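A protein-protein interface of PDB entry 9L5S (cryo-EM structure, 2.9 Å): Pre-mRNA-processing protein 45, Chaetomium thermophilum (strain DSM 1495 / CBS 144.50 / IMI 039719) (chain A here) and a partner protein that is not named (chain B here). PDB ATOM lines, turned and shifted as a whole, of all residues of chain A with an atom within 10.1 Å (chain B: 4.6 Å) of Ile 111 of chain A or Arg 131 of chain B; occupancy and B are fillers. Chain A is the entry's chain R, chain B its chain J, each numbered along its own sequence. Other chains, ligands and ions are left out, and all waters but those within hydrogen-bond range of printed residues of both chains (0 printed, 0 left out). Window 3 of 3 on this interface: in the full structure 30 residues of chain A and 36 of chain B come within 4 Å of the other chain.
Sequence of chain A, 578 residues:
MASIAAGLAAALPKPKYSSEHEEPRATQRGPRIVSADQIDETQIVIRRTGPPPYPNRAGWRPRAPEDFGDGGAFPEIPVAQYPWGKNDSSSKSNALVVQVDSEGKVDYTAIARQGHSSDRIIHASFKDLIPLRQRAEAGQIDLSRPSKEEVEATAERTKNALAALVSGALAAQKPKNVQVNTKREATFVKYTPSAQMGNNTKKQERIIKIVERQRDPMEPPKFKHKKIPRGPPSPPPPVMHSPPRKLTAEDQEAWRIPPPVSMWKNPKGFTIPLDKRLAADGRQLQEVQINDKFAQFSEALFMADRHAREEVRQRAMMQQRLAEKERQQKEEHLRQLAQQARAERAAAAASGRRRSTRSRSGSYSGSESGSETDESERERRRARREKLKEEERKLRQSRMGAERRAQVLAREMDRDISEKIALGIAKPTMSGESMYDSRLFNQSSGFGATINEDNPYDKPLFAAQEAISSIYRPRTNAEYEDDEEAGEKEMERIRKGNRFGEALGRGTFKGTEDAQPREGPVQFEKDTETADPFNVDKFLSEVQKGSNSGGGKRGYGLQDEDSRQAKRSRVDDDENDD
Tyr 108 of chain A touches Asp 130 of chain B.
CB of Asp 130 of chain B touches CD1 of Ile 111 of chain A (3.9 Å).
Arg 131 of chain B touches Ile 111 of chain A.
Thr 134 of chain B touches Ile 111 of chain A (OG1 to CG2, 3.9 Å).
Ala 112 of chain A touches Thr 134 of chain B (CB to CG2, 3.7 Å).
Arg 135 of chain B touches Pro 236 of chain A (CZ to CG, 3.5 Å).
CB of Pro 238 of chain A touches O of Thr 134 of chain B, 3.2 Å away.
Pro 238 of chain A touches Arg 135 of chain B.
The backbone NH (N) of Val 239 of chain A is in hydrogen-bond range of the backbone carbonyl oxygen (O) of Arg 135 of chain B.
Of the 12 printed residues of chain B, 4 touch a printed residue of chain A.
Printed residues of chain B that touch a printed residue of chain A: Asp 130, Arg 131, Thr 134 and Arg 135.
Of the 25 printed residues of chain A, 6 touch a printed residue of chain B.
Along chain A the printed residues that touch a printed residue of chain B span positions 108 to 239.
Among the printed residues, 9 pairs touch across the chains.
The guanidinium group (NH1) of Arg 131 of chain B is in salt-bridge range of the side-chain carboxylate (OE2) of Glu 96 of chain B (2.4 Å).
The backbone carbonyl oxygen (O) of Asp 130 of chain B is in hydrogen-bond range of the side-chain hydroxyl (OG1) of Thr 134 of chain B (2.7 Å).
Printed residues of chain B within 4 Å of Ile 111 of chain A: Asp 130 (3.9 Å), Arg 131 (3.9 Å) and Thr 134 (3.9 Å).
Of chain A, only Ile 111 comes within 4 Å of Arg 131 of chain B.
No residue of chain A comes within 4 Å of Leu 128 of chain B.
No residue of chain A comes within 4 Å of Ala 132 of chain B.
Of the printed residues of chain B, Ala 112 of chain A touches Thr 134 (3.7 Å).
Printed residues of chain A within 4 Å of Arg 135 of chain B: Pro 236 (3.5 Å), Pro 238 (3.4 Å) and Val 239 (2.7 Å).
Printed residues of chain B within 4 Å of Tyr 108 of chain A: Asp 130.
Printed residues of chain A within 4 Å of Asp 130 of chain B: Tyr 108 and Ile 111.
Val 98 of chain A touches none of the printed residues of chain B.
The nearest printed residue of chain B that does not touch Pro 236 of chain A is Leu 99 of chain B (5.3 Å).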
ATOM      1  N   ALA A  95      16.909  29.039 -13.940  1.00  0.00           N
ATOM      2  CA  ALA A  95      16.951  27.590 -14.023  1.00  0.00           C
ATOM      3  C   ALA A  95      18.307  27.124 -14.548  1.00  0.00           C
ATOM      4  O   ALA A  95      19.113  27.907 -15.059  1.00  0.00           O
ATOM      5  CB  ALA A  95      15.824  27.070 -14.913  1.00  0.00           C
ATOM      6  N   LEU A  96      18.557  25.828 -14.411  1.00  0.00           N
ATOM      7  CA  LEU A  96      19.786  25.222 -14.896  1.00  0.00           C
ATOM      8  C   LEU A  96      19.641  24.780 -16.346  1.00  0.00           C
ATOM      9  O   LEU A  96      18.538  24.586 -16.861  1.00  0.00           O
ATOM     10  CB  LEU A  96      20.191  24.025 -14.033  1.00  0.00           C
ATOM     11  CG  LEU A  96      21.110  24.257 -12.831  1.00  0.00           C
ATOM     12  CD1 LEU A  96      20.442  25.072 -11.752  1.00  0.00           C
ATOM     13  CD2 LEU A  96      21.574  22.923 -12.274  1.00  0.00           C
ATOM     14  N   VAL A  97      20.788  24.622 -17.001  1.00  0.00           N
ATOM     15  CA  VAL A  97      20.826  24.127 -18.370  1.00  0.00           C
ATOM     16  C   VAL A  97      20.507  22.638 -18.361  1.00  0.00           C
ATOM     17  O   VAL A  97      21.230  21.836 -17.758  1.00  0.00           O
ATOM     18  CB  VAL A  97      22.192  24.403 -19.008  1.00  0.00           C
ATOM     19  CG1 VAL A  97      22.308  23.698 -20.337  1.00  0.00           C
ATOM     20  CG2 VAL A  97      22.394  25.899 -19.183  1.00  0.00           C
ATOM     21  N   VAL A  98      19.422  22.262 -19.031  1.00  0.00           N
ATOM     22  CA  VAL A  98      18.977  20.873 -19.050  1.00  0.00           C
ATOM     23  C   VAL A  98      19.792  20.115 -20.090  1.00  0.00           C
ATOM     24  O   VAL A  98      19.805  20.479 -21.270  1.00  0.00           O
ATOM     25  CB  VAL A  98      17.472  20.779 -19.343  1.00  0.00           C
ATOM     26  CG1 VAL A  98      17.093  19.372 -19.787  1.00  0.00           C
ATOM     27  CG2 VAL A  98      16.668  21.190 -18.123  1.00  0.00           C
ATOM     28  N   GLN A  99      20.484  19.070 -19.650  1.00  0.00           N
ATOM     29  CA  GLN A  99      21.281  18.227 -20.526  1.00  0.00           C
ATOM     30  C   GLN A  99      20.607  16.875 -20.723  1.00  0.00           C
ATOM     31  O   GLN A  99      19.653  16.517 -20.028  1.00  0.00           O
ATOM     32  CB  GLN A  99      22.690  18.037 -19.957  1.00  0.00           C
ATOM     33  CG  GLN A  99      23.553  19.284 -19.988  1.00  0.00           C
ATOM     34  CD  GLN A  99      25.020  18.976 -19.760  1.00  0.00           C
ATOM     35  OE1 GLN A  99      25.376  17.882 -19.321  1.00  0.00           O
ATOM     36  NE2 GLN A  99      25.881  19.940 -20.063  1.00  0.00           N
ATOM     37  N   VAL A 106      16.564  12.968 -19.462  1.00  0.00           N
ATOM     38  CA  VAL A 106      16.961  14.177 -18.749  1.00  0.00           C
ATOM     39  C   VAL A 106      18.014  13.812 -17.712  1.00  0.00           C
ATOM     40  O   VAL A 106      17.798  12.934 -16.869  1.00  0.00           O
ATOM     41  CB  VAL A 106      15.750  14.860 -18.101  1.00  0.00           C
ATOM     42  CG1 VAL A 106      16.155  16.199 -17.509  1.00  0.00           C
ATOM     43  CG2 VAL A 106      14.643  15.043 -19.122  1.00  0.00           C
ATOM     44  N   ASP A 107      19.165  14.473 -17.779  1.00  0.00           N
ATOM     45  CA  ASP A 107      20.272  14.169 -16.884  1.00  0.00           C
ATOM     46  C   ASP A 107      20.070  14.897 -15.561  1.00  0.00           C
ATOM     47  O   ASP A 107      19.949  16.124 -15.529  1.00  0.00           O
ATOM     48  CB  ASP A 107      21.598  14.576 -17.525  1.00  0.00           C
ATOM     49  CG  ASP A 107      22.808  14.041 -16.775  1.00  0.00           C
ATOM     50  OD1 ASP A 107      22.633  13.252 -15.822  1.00  0.00           O
ATOM     51  OD2 ASP A 107      23.942  14.413 -17.143  1.00  0.00           O
ATOM     52  N   TYR A 108      20.040  14.135 -14.469  1.00  0.00           N
ATOM     53  CA  TYR A 108      19.800  14.684 -13.141  1.00  0.00           C
ATOM     54  C   TYR A 108      21.053  14.700 -12.278  1.00  0.00           C
ATOM     55  O   TYR A 108      20.955  14.919 -11.065  1.00  0.00           O
ATOM     56  CB  TYR A 108      18.683  13.907 -12.447  1.00  0.00           C
ATOM     57  CG  TYR A 108      17.310  14.269 -12.961  1.00  0.00           C
ATOM     58  CD1 TYR A 108      16.642  15.386 -12.480  1.00  0.00           C
ATOM     59  CD2 TYR A 108      16.694  13.507 -13.943  1.00  0.00           C
ATOM     60  CE1 TYR A 108      15.391  15.725 -12.952  1.00  0.00           C
ATOM     61  CE2 TYR A 108      15.446  13.840 -14.424  1.00  0.00           C
ATOM     62  CZ  TYR A 108      14.799  14.948 -13.924  1.00  0.00           C
ATOM     63  OH  TYR A 108      13.553  15.282 -14.399  1.00  0.00           O
ATOM     64  N   THR A 109      22.225  14.479 -12.867  1.00  0.00           N
ATOM     65  CA  THR A 109      23.472  14.550 -12.119  1.00  0.00           C
ATOM     66  C   THR A 109      23.978  15.976 -11.954  1.00  0.00           C
ATOM     67  O   THR A 109      24.985  16.182 -11.273  1.00  0.00           O
ATOM     68  CB  THR A 109      24.548  13.701 -12.799  1.00  0.00           C
ATOM     69  OG1 THR A 109      24.637  14.060 -14.183  1.00  0.00           O
ATOM     70  CG2 THR A 109      24.212  12.220 -12.681  1.00  0.00           C
ATOM     71  N   ALA A 110      23.308  16.959 -12.559  1.00  0.00           N
ATOM     72  CA  ALA A 110      23.665  18.354 -12.336  1.00  0.00           C
ATOM     73  C   ALA A 110      23.193  18.855 -10.981  1.00  0.00           C
ATOM     74  O   ALA A 110      23.648  19.910 -10.530  1.00  0.00           O
ATOM     75  CB  ALA A 110      23.085  19.231 -13.446  1.00  0.00           C
ATOM     76  N   ILE A 111      22.293  18.125 -10.329  1.00  0.00           N
ATOM     77  CA  ILE A 111      21.809  18.495  -9.004  1.00  0.00           C
ATOM     78  C   ILE A 111      22.742  17.983  -7.914  1.00  0.00           C
ATOM     79  O   ILE A 111      23.023  18.694  -6.946  1.00  0.00           O
ATOM     80  CB  ILE A 111      20.373  17.967  -8.814  1.00  0.00           C
ATOM     81  CG1 ILE A 111      19.495  18.389  -9.993  1.00  0.00           C
ATOM     82  CG2 ILE A 111      19.781  18.466  -7.508  1.00  0.00           C
ATOM     83  CD1 ILE A 111      18.136  17.734 -10.005  1.00  0.00           C
ATOM     84  N   ALA A 112      23.240  16.753  -8.062  1.00  0.00           N
ATOM     85  CA  ALA A 112      24.193  16.215  -7.098  1.00  0.00           C
ATOM     86  C   ALA A 112      25.554  16.884  -7.217  1.00  0.00           C
ATOM     87  O   ALA A 112      26.258  17.039  -6.214  1.00  0.00           O
ATOM     88  CB  ALA A 112      24.332  14.706  -7.283  1.00  0.00           C
ATOM     89  N   ARG A 113      25.940  17.284  -8.425  1.00  0.00           N
ATOM     90  CA  ARG A 113      27.241  17.887  -8.672  1.00  0.00           C
ATOM     91  C   ARG A 113      27.214  19.401  -8.486  1.00  0.00           C
ATOM     92  O   ARG A 113      28.236  20.064  -8.690  1.00  0.00           O
ATOM     93  CB  ARG A 113      27.709  17.523 -10.089  1.00  0.00           C
ATOM     94  CG  ARG A 113      29.212  17.563 -10.324  1.00  0.00           C
ATOM     95  CD  ARG A 113      29.610  16.623 -11.451  1.00  0.00           C
ATOM     96  NE  ARG A 113      30.055  15.321 -10.968  1.00  0.00           N
ATOM     97  CZ  ARG A 113      31.236  15.080 -10.417  1.00  0.00           C
ATOM     98  NH1 ARG A 113      32.137  16.035 -10.259  1.00  0.00           N
ATOM     99  NH2 ARG A 113      31.526  13.845 -10.020  1.00  0.00           N
ATOM    100  N   GLN A 114      26.075  19.957  -8.079  1.00  0.00           N
ATOM    101  CA  GLN A 114      25.928  21.402  -7.953  1.00  0.00           C
ATOM    102  C   GLN A 114      26.730  21.912  -6.762  1.00  0.00           C
ATOM    103  O   GLN A 114      26.515  21.478  -5.626  1.00  0.00           O
ATOM    104  CB  GLN A 114      24.452  21.758  -7.800  1.00  0.00           C
ATOM    105  CG  GLN A 114      24.142  23.230  -7.972  1.00  0.00           C
ATOM    106  CD  GLN A 114      22.654  23.493  -8.076  1.00  0.00           C
ATOM    107  OE1 GLN A 114      21.846  22.565  -8.067  1.00  0.00           O
ATOM    108  NE2 GLN A 114      22.285  24.761  -8.177  1.00  0.00           N
ATOM    109  N   GLY A 115      27.652  22.835  -7.024  1.00  0.00           N
ATOM    110  CA  GLY A 115      28.531  23.356  -6.001  1.00  0.00           C
ATOM    111  C   GLY A 115      29.859  22.644  -5.876  1.00  0.00           C
ATOM    112  O   GLY A 115      30.648  22.994  -4.990  1.00  0.00           O
ATOM    113  N   HIS A 116      30.132  21.662  -6.729  1.00  0.00           N
ATOM    114  CA  HIS A 116      31.352  20.875  -6.669  1.00  0.00           C
ATOM    115  C   HIS A 116      32.128  21.017  -7.971  1.00  0.00           C
ATOM    116  O   HIS A 116      31.552  21.283  -9.030  1.00  0.00           O
ATOM    117  CB  HIS A 116      31.044  19.395  -6.409  1.00  0.00           C
ATOM    118  CG  HIS A 116      30.747  19.081  -4.976  1.00  0.00           C
ATOM    119  ND1 HIS A 116      31.685  19.214  -3.976  1.00  0.00           N
ATOM    120  CD2 HIS A 116      29.617  18.642  -4.376  1.00  0.00           C
ATOM    121  CE1 HIS A 116      31.145  18.870  -2.821  1.00  0.00           C
ATOM    122  NE2 HIS A 116      29.891  18.517  -3.036  1.00  0.00           N
ATOM    123  N   ILE A 122      31.589  11.905  -7.202  1.00  0.00           N
ATOM    124  CA  ILE A 122      30.258  11.883  -6.607  1.00  0.00           C
ATOM    125  C   ILE A 122      29.503  10.687  -7.167  1.00  0.00           C
ATOM    126  O   ILE A 122      29.310  10.587  -8.384  1.00  0.00           O
ATOM    127  CB  ILE A 122      29.476  13.181  -6.876  1.00  0.00           C
ATOM    128  CG1 ILE A 122      30.286  14.407  -6.445  1.00  0.00           C
ATOM    129  CG2 ILE A 122      28.133  13.151  -6.165  1.00  0.00           C
ATOM    130  CD1 ILE A 122      29.571  15.717  -6.639  1.00  0.00           C
ATOM    131  N   HIS A 123      29.084   9.782  -6.288  1.00  0.00           N
ATOM    132  CA  HIS A 123      28.201   8.685  -6.662  1.00  0.00           C
ATOM    133  C   HIS A 123      26.762   9.174  -6.563  1.00  0.00           C
ATOM    134  O   HIS A 123      26.313   9.569  -5.482  1.00  0.00           O
ATOM    135  CB  HIS A 123      28.421   7.473  -5.757  1.00  0.00           C
ATOM    136  CG  HIS A 123      29.761   6.827  -5.923  1.00  0.00           C
ATOM    137  ND1 HIS A 123      30.657   7.209  -6.899  1.00  0.00           N
ATOM    138  CD2 HIS A 123      30.358   5.825  -5.237  1.00  0.00           C
ATOM    139  CE1 HIS A 123      31.748   6.469  -6.805  1.00  0.00           C
ATOM    140  NE2 HIS A 123      31.592   5.622  -5.804  1.00  0.00           N
ATOM    141  N   ALA A 124      26.039   9.148  -7.684  1.00  0.00           N
ATOM    142  CA  ALA A 124      24.703   9.730  -7.709  1.00  0.00           C
ATOM    143  C   ALA A 124      23.682   8.896  -8.476  1.00  0.00           C
ATOM    144  O   ALA A 124      22.569   9.383  -8.708  1.00  0.00           O
ATOM    145  CB  ALA A 124      24.751  11.143  -8.298  1.00  0.00           C
ATOM    146  N   SER A 234      30.850  21.755   2.359  1.00  0.00           N
ATOM    147  CA  SER A 234      30.692  21.406   0.958  1.00  0.00           C
ATOM    148  C   SER A 234      29.351  20.696   0.758  1.00  0.00           C
ATOM    149  O   SER A 234      28.840  20.064   1.688  1.00  0.00           O
ATOM    150  CB  SER A 234      31.850  20.518   0.504  1.00  0.00           C
ATOM    151  OG  SER A 234      32.145  19.521   1.468  1.00  0.00           O
ATOM    152  N   PRO A 235      28.738  20.831  -0.421  1.00  0.00           N
ATOM    153  CA  PRO A 235      27.421  20.207  -0.664  1.00  0.00           C
ATOM    154  C   PRO A 235      27.482  18.700  -0.500  1.00  0.00           C
ATOM    155  O   PRO A 235      28.287  18.026  -1.159  1.00  0.00           O
ATOM    156  CB  PRO A 235      27.104  20.601  -2.114  1.00  0.00           C
ATOM    157  CG  PRO A 235      27.907  21.826  -2.354  1.00  0.00           C
ATOM    158  CD  PRO A 235      29.164  21.661  -1.562  1.00  0.00           C
ATOM    159  N   PRO A 236      26.662  18.144   0.399  1.00  0.00           N
ATOM    160  CA  PRO A 236      26.827  16.739   0.769  1.00  0.00           C
ATOM    161  C   PRO A 236      26.413  15.818  -0.363  1.00  0.00           C
ATOM    162  O   PRO A 236      25.533  16.157  -1.172  1.00  0.00           O
ATOM    163  CB  PRO A 236      25.903  16.581   1.990  1.00  0.00           C
ATOM    164  CG  PRO A 236      25.014  17.758   1.980  1.00  0.00           C
ATOM    165  CD  PRO A 236      25.714  18.854   1.273  1.00  0.00           C
ATOM    166  N   PRO A 237      27.024  14.640  -0.462  1.00  0.00           N
ATOM    167  CA  PRO A 237      26.741  13.736  -1.580  1.00  0.00           C
ATOM    168  C   PRO A 237      25.410  13.031  -1.394  1.00  0.00           C
ATOM    169  O   PRO A 237      24.807  13.101  -0.312  1.00  0.00           O
ATOM    170  CB  PRO A 237      27.910  12.742  -1.519  1.00  0.00           C
ATOM    171  CG  PRO A 237      28.289  12.730  -0.092  1.00  0.00           C
ATOM    172  CD  PRO A 237      28.127  14.141   0.375  1.00  0.00           C
ATOM    173  N   PRO A 238      24.907  12.361  -2.434  1.00  0.00           N
ATOM    174  CA  PRO A 238      23.747  11.482  -2.251  1.00  0.00           C
ATOM    175  C   PRO A 238      24.054  10.332  -1.303  1.00  0.00           C
ATOM    176  O   PRO A 238      25.187   9.857  -1.210  1.00  0.00           O
ATOM    177  CB  PRO A 238      23.461  10.975  -3.667  1.00  0.00           C
ATOM    178  CG  PRO A 238      24.001  12.034  -4.552  1.00  0.00           C
ATOM    179  CD  PRO A 238      25.213  12.568  -3.861  1.00  0.00           C
ATOM    180  N   VAL A 239      23.021   9.890  -0.594  1.00  0.00           N
ATOM    181  CA  VAL A 239      23.150   8.837   0.407  1.00  0.00           C
ATOM    182  C   VAL A 239      22.871   7.504  -0.277  1.00  0.00           C
ATOM    183  O   VAL A 239      21.727   7.195  -0.621  1.00  0.00           O
ATOM    184  CB  VAL A 239      22.205   9.073   1.587  1.00  0.00           C
ATOM    185  CG1 VAL A 239      22.396   8.008   2.618  1.00  0.00           C
ATOM    186  CG2 VAL A 239      22.471  10.425   2.190  1.00  0.00           C
ATOM    187  N   GLU B  96      17.490  26.262   4.692  1.00  0.00           N
ATOM    188  CA  GLU B  96      18.722  25.816   4.046  1.00  0.00           C
ATOM    189  C   GLU B  96      19.880  25.718   5.032  1.00  0.00           C
ATOM    190  O   GLU B  96      20.730  24.832   4.896  1.00  0.00           O
ATOM    191  CB  GLU B  96      19.085  26.739   2.883  1.00  0.00           C
ATOM    192  CG  GLU B  96      18.138  26.654   1.700  1.00  0.00           C
ATOM    193  CD  GLU B  96      18.508  25.544   0.742  1.00  0.00           C
ATOM    194  OE1 GLU B  96      19.713  25.246   0.617  1.00  0.00           O
ATOM    195  OE2 GLU B  96      17.595  24.967   0.112  1.00  0.00           O
ATOM    196  N   LEU B  99      19.276  22.495   6.681  1.00  0.00           N
ATOM    197  CA  LEU B  99      19.754  21.465   5.770  1.00  0.00           C
ATOM    198  C   LEU B  99      21.271  21.384   5.729  1.00  0.00           C
ATOM    199  O   LEU B  99      21.810  20.324   5.404  1.00  0.00           O
ATOM    200  CB  LEU B  99      19.215  21.720   4.363  1.00  0.00           C
ATOM    201  CG  LEU B  99      17.826  21.162   4.066  1.00  0.00           C
ATOM    202  CD1 LEU B  99      17.372  21.574   2.677  1.00  0.00           C
ATOM    203  CD2 LEU B  99      17.837  19.656   4.206  1.00  0.00           C
ATOM    204  N   TRP B 109      13.324  17.770   5.268  1.00  0.00           N
ATOM    205  CA  TRP B 109      13.025  17.867   3.843  1.00  0.00           C
ATOM    206  C   TRP B 109      11.523  17.902   3.594  1.00  0.00           C
ATOM    207  O   TRP B 109      11.040  18.713   2.795  1.00  0.00           O
ATOM    208  CB  TRP B 109      13.645  16.688   3.089  1.00  0.00           C
ATOM    209  CG  TRP B 109      15.068  16.875   2.650  1.00  0.00           C
ATOM    210  CD1 TRP B 109      16.162  16.210   3.121  1.00  0.00           C
ATOM    211  CD2 TRP B 109      15.548  17.768   1.639  1.00  0.00           C
ATOM    212  NE1 TRP B 109      17.294  16.638   2.472  1.00  0.00           N
ATOM    213  CE2 TRP B 109      16.943  17.592   1.555  1.00  0.00           C
ATOM    214  CE3 TRP B 109      14.936  18.703   0.799  1.00  0.00           C
ATOM    215  CZ2 TRP B 109      17.736  18.319   0.671  1.00  0.00           C
ATOM    216  CZ3 TRP B 109      15.725  19.419  -0.082  1.00  0.00           C
ATOM    217  CH2 TRP B 109      17.109  19.224  -0.138  1.00  0.00           C
ATOM    218  N   ASN B 127      11.846  21.960  -7.454  1.00  0.00           N
ATOM    219  CA  ASN B 127      13.302  21.941  -7.333  1.00  0.00           C
ATOM    220  C   ASN B 127      13.727  21.303  -6.016  1.00  0.00           C
ATOM    221  O   ASN B 127      14.709  20.551  -5.958  1.00  0.00           O
ATOM    222  CB  ASN B 127      13.850  23.365  -7.428  1.00  0.00           C
ATOM    223  CG  ASN B 127      13.857  23.892  -8.842  1.00  0.00           C
ATOM    224  OD1 ASN B 127      13.670  23.143  -9.797  1.00  0.00           O
ATOM    225  ND2 ASN B 127      14.076  25.194  -8.984  1.00  0.00           N
ATOM    226  N   LEU B 128      12.978  21.586  -4.951  1.00  0.00           N
ATOM    227  CA  LEU B 128      13.281  21.048  -3.632  1.00  0.00           C
ATOM    228  C   LEU B 128      13.092  19.540  -3.594  1.00  0.00           C
ATOM    229  O   LEU B 128      13.890  18.822  -2.987  1.00  0.00           O
ATOM    230  CB  LEU B 128      12.381  21.715  -2.602  1.00  0.00           C
ATOM    231  CG  LEU B 128      12.847  23.123  -2.256  1.00  0.00           C
ATOM    232  CD1 LEU B 128      12.007  23.695  -1.126  1.00  0.00           C
ATOM    233  CD2 LEU B 128      14.352  23.182  -2.008  1.00  0.00           C
ATOM    234  N   LEU B 129      12.032  19.051  -4.234  1.00  0.00           N
ATOM    235  CA  LEU B 129      11.791  17.617  -4.316  1.00  0.00           C
ATOM    236  C   LEU B 129      12.829  16.921  -5.182  1.00  0.00           C
ATOM    237  O   LEU B 129      13.209  15.783  -4.888  1.00  0.00           O
ATOM    238  CB  LEU B 129      10.388  17.368  -4.855  1.00  0.00           C
ATOM    239  CG  LEU B 129       9.234  17.558  -3.872  1.00  0.00           C
ATOM    240  CD1 LEU B 129       7.964  17.993  -4.579  1.00  0.00           C
ATOM    241  CD2 LEU B 129       8.989  16.268  -3.111  1.00  0.00           C
ATOM    242  N   ASP B 130      13.301  17.587  -6.241  1.00  0.00           N
ATOM    243  CA  ASP B 130      14.409  17.042  -7.020  1.00  0.00           C
ATOM    244  C   ASP B 130      15.668  16.916  -6.171  1.00  0.00           C
ATOM    245  O   ASP B 130      16.347  15.883  -6.206  1.00  0.00           O
ATOM    246  CB  ASP B 130      14.673  17.919  -8.242  1.00  0.00           C
ATOM    247  CG  ASP B 130      13.848  17.507  -9.441  1.00  0.00           C
ATOM    248  OD1 ASP B 130      13.301  16.386  -9.428  1.00  0.00           O
ATOM    249  OD2 ASP B 130      13.748  18.305 -10.396  1.00  0.00           O
ATOM    250  N   ARG B 131      15.973  17.948  -5.378  1.00  0.00           N
ATOM    251  CA  ARG B 131      17.112  17.885  -4.464  1.00  0.00           C
ATOM    252  C   ARG B 131      16.931  16.792  -3.415  1.00  0.00           C
ATOM    253  O   ARG B 131      17.893  16.104  -3.051  1.00  0.00           O
ATOM    254  CB  ARG B 131      17.309  19.239  -3.781  1.00  0.00           C
ATOM    255  CG  ARG B 131      17.919  20.317  -4.655  1.00  0.00           C
ATOM    256  CD  ARG B 131      17.912  21.645  -3.922  1.00  0.00           C
ATOM    257  NE  ARG B 131      18.740  21.606  -2.724  1.00  0.00           N
ATOM    258  CZ  ARG B 131      18.753  22.548  -1.791  1.00  0.00           C
ATOM    259  NH1 ARG B 131      17.991  23.625  -1.887  1.00  0.00           N
ATOM    260  NH2 ARG B 131      19.545  22.404  -0.733  1.00  0.00           N
ATOM    261  N   ALA B 132      15.703  16.623  -2.919  1.00  0.00           N
ATOM    262  CA  ALA B 132      15.437  15.651  -1.864  1.00  0.00           C
ATOM    263  C   ALA B 132      15.560  14.221  -2.368  1.00  0.00           C
ATOM    264  O   ALA B 132      16.107  13.359  -1.672  1.00  0.00           O
ATOM    265  CB  ALA B 132      14.049  15.889  -1.277  1.00  0.00           C
ATOM    266  N   VAL B 133      15.055  13.941  -3.573  1.00  0.00           N
ATOM    267  CA  VAL B 133      15.216  12.599  -4.129  1.00  0.00           C
ATOM    268  C   VAL B 133      16.601  12.381  -4.712  1.00  0.00           C
ATOM    269  O   VAL B 133      16.986  11.231  -4.950  1.00  0.00           O
ATOM    270  CB  VAL B 133      14.160  12.284  -5.206  1.00  0.00           C
ATOM    271  CG1 VAL B 133      12.760  12.499  -4.657  1.00  0.00           C
ATOM    272  CG2 VAL B 133      14.390  13.120  -6.452  1.00  0.00           C
ATOM    273  N   THR B 134      17.363  13.451  -4.950  1.00  0.00           N
ATOM    274  CA  THR B 134      18.768  13.278  -5.297  1.00  0.00           C
ATOM    275  C   THR B 134      19.590  12.909  -4.068  1.00  0.00           C
ATOM    276  O   THR B 134      20.420  11.995  -4.123  1.00  0.00           O
ATOM    277  CB  THR B 134      19.304  14.554  -5.947  1.00  0.00           C
ATOM    278  OG1 THR B 134      18.623  14.779  -7.188  1.00  0.00           O
ATOM    279  CG2 THR B 134      20.789  14.438  -6.219  1.00  0.00           C
ATOM    280  N   ARG B 135      19.350  13.589  -2.943  1.00  0.00           N
ATOM    281  CA  ARG B 135      20.144  13.346  -1.742  1.00  0.00           C
ATOM    282  C   ARG B 135      19.811  12.001  -1.112  1.00  0.00           C
ATOM    283  O   ARG B 135      20.712  11.258  -0.705  1.00  0.00           O
ATOM    284  CB  ARG B 135      19.932  14.475  -0.732  1.00  0.00           C
ATOM    285  CG  ARG B 135      20.542  14.199   0.634  1.00  0.00           C
ATOM    286  CD  ARG B 135      21.156  15.444   1.240  1.00  0.00           C
ATOM    287  NE  ARG B 135      21.913  16.224   0.272  1.00  0.00           N
ATOM    288  CZ  ARG B 135      21.992  17.547   0.284  1.00  0.00           C
ATOM    289  NH1 ARG B 135      21.383  18.265   1.213  1.00  0.00           N
ATOM    290  NH2 ARG B 135      22.705  18.163  -0.653  1.00  0.00           N
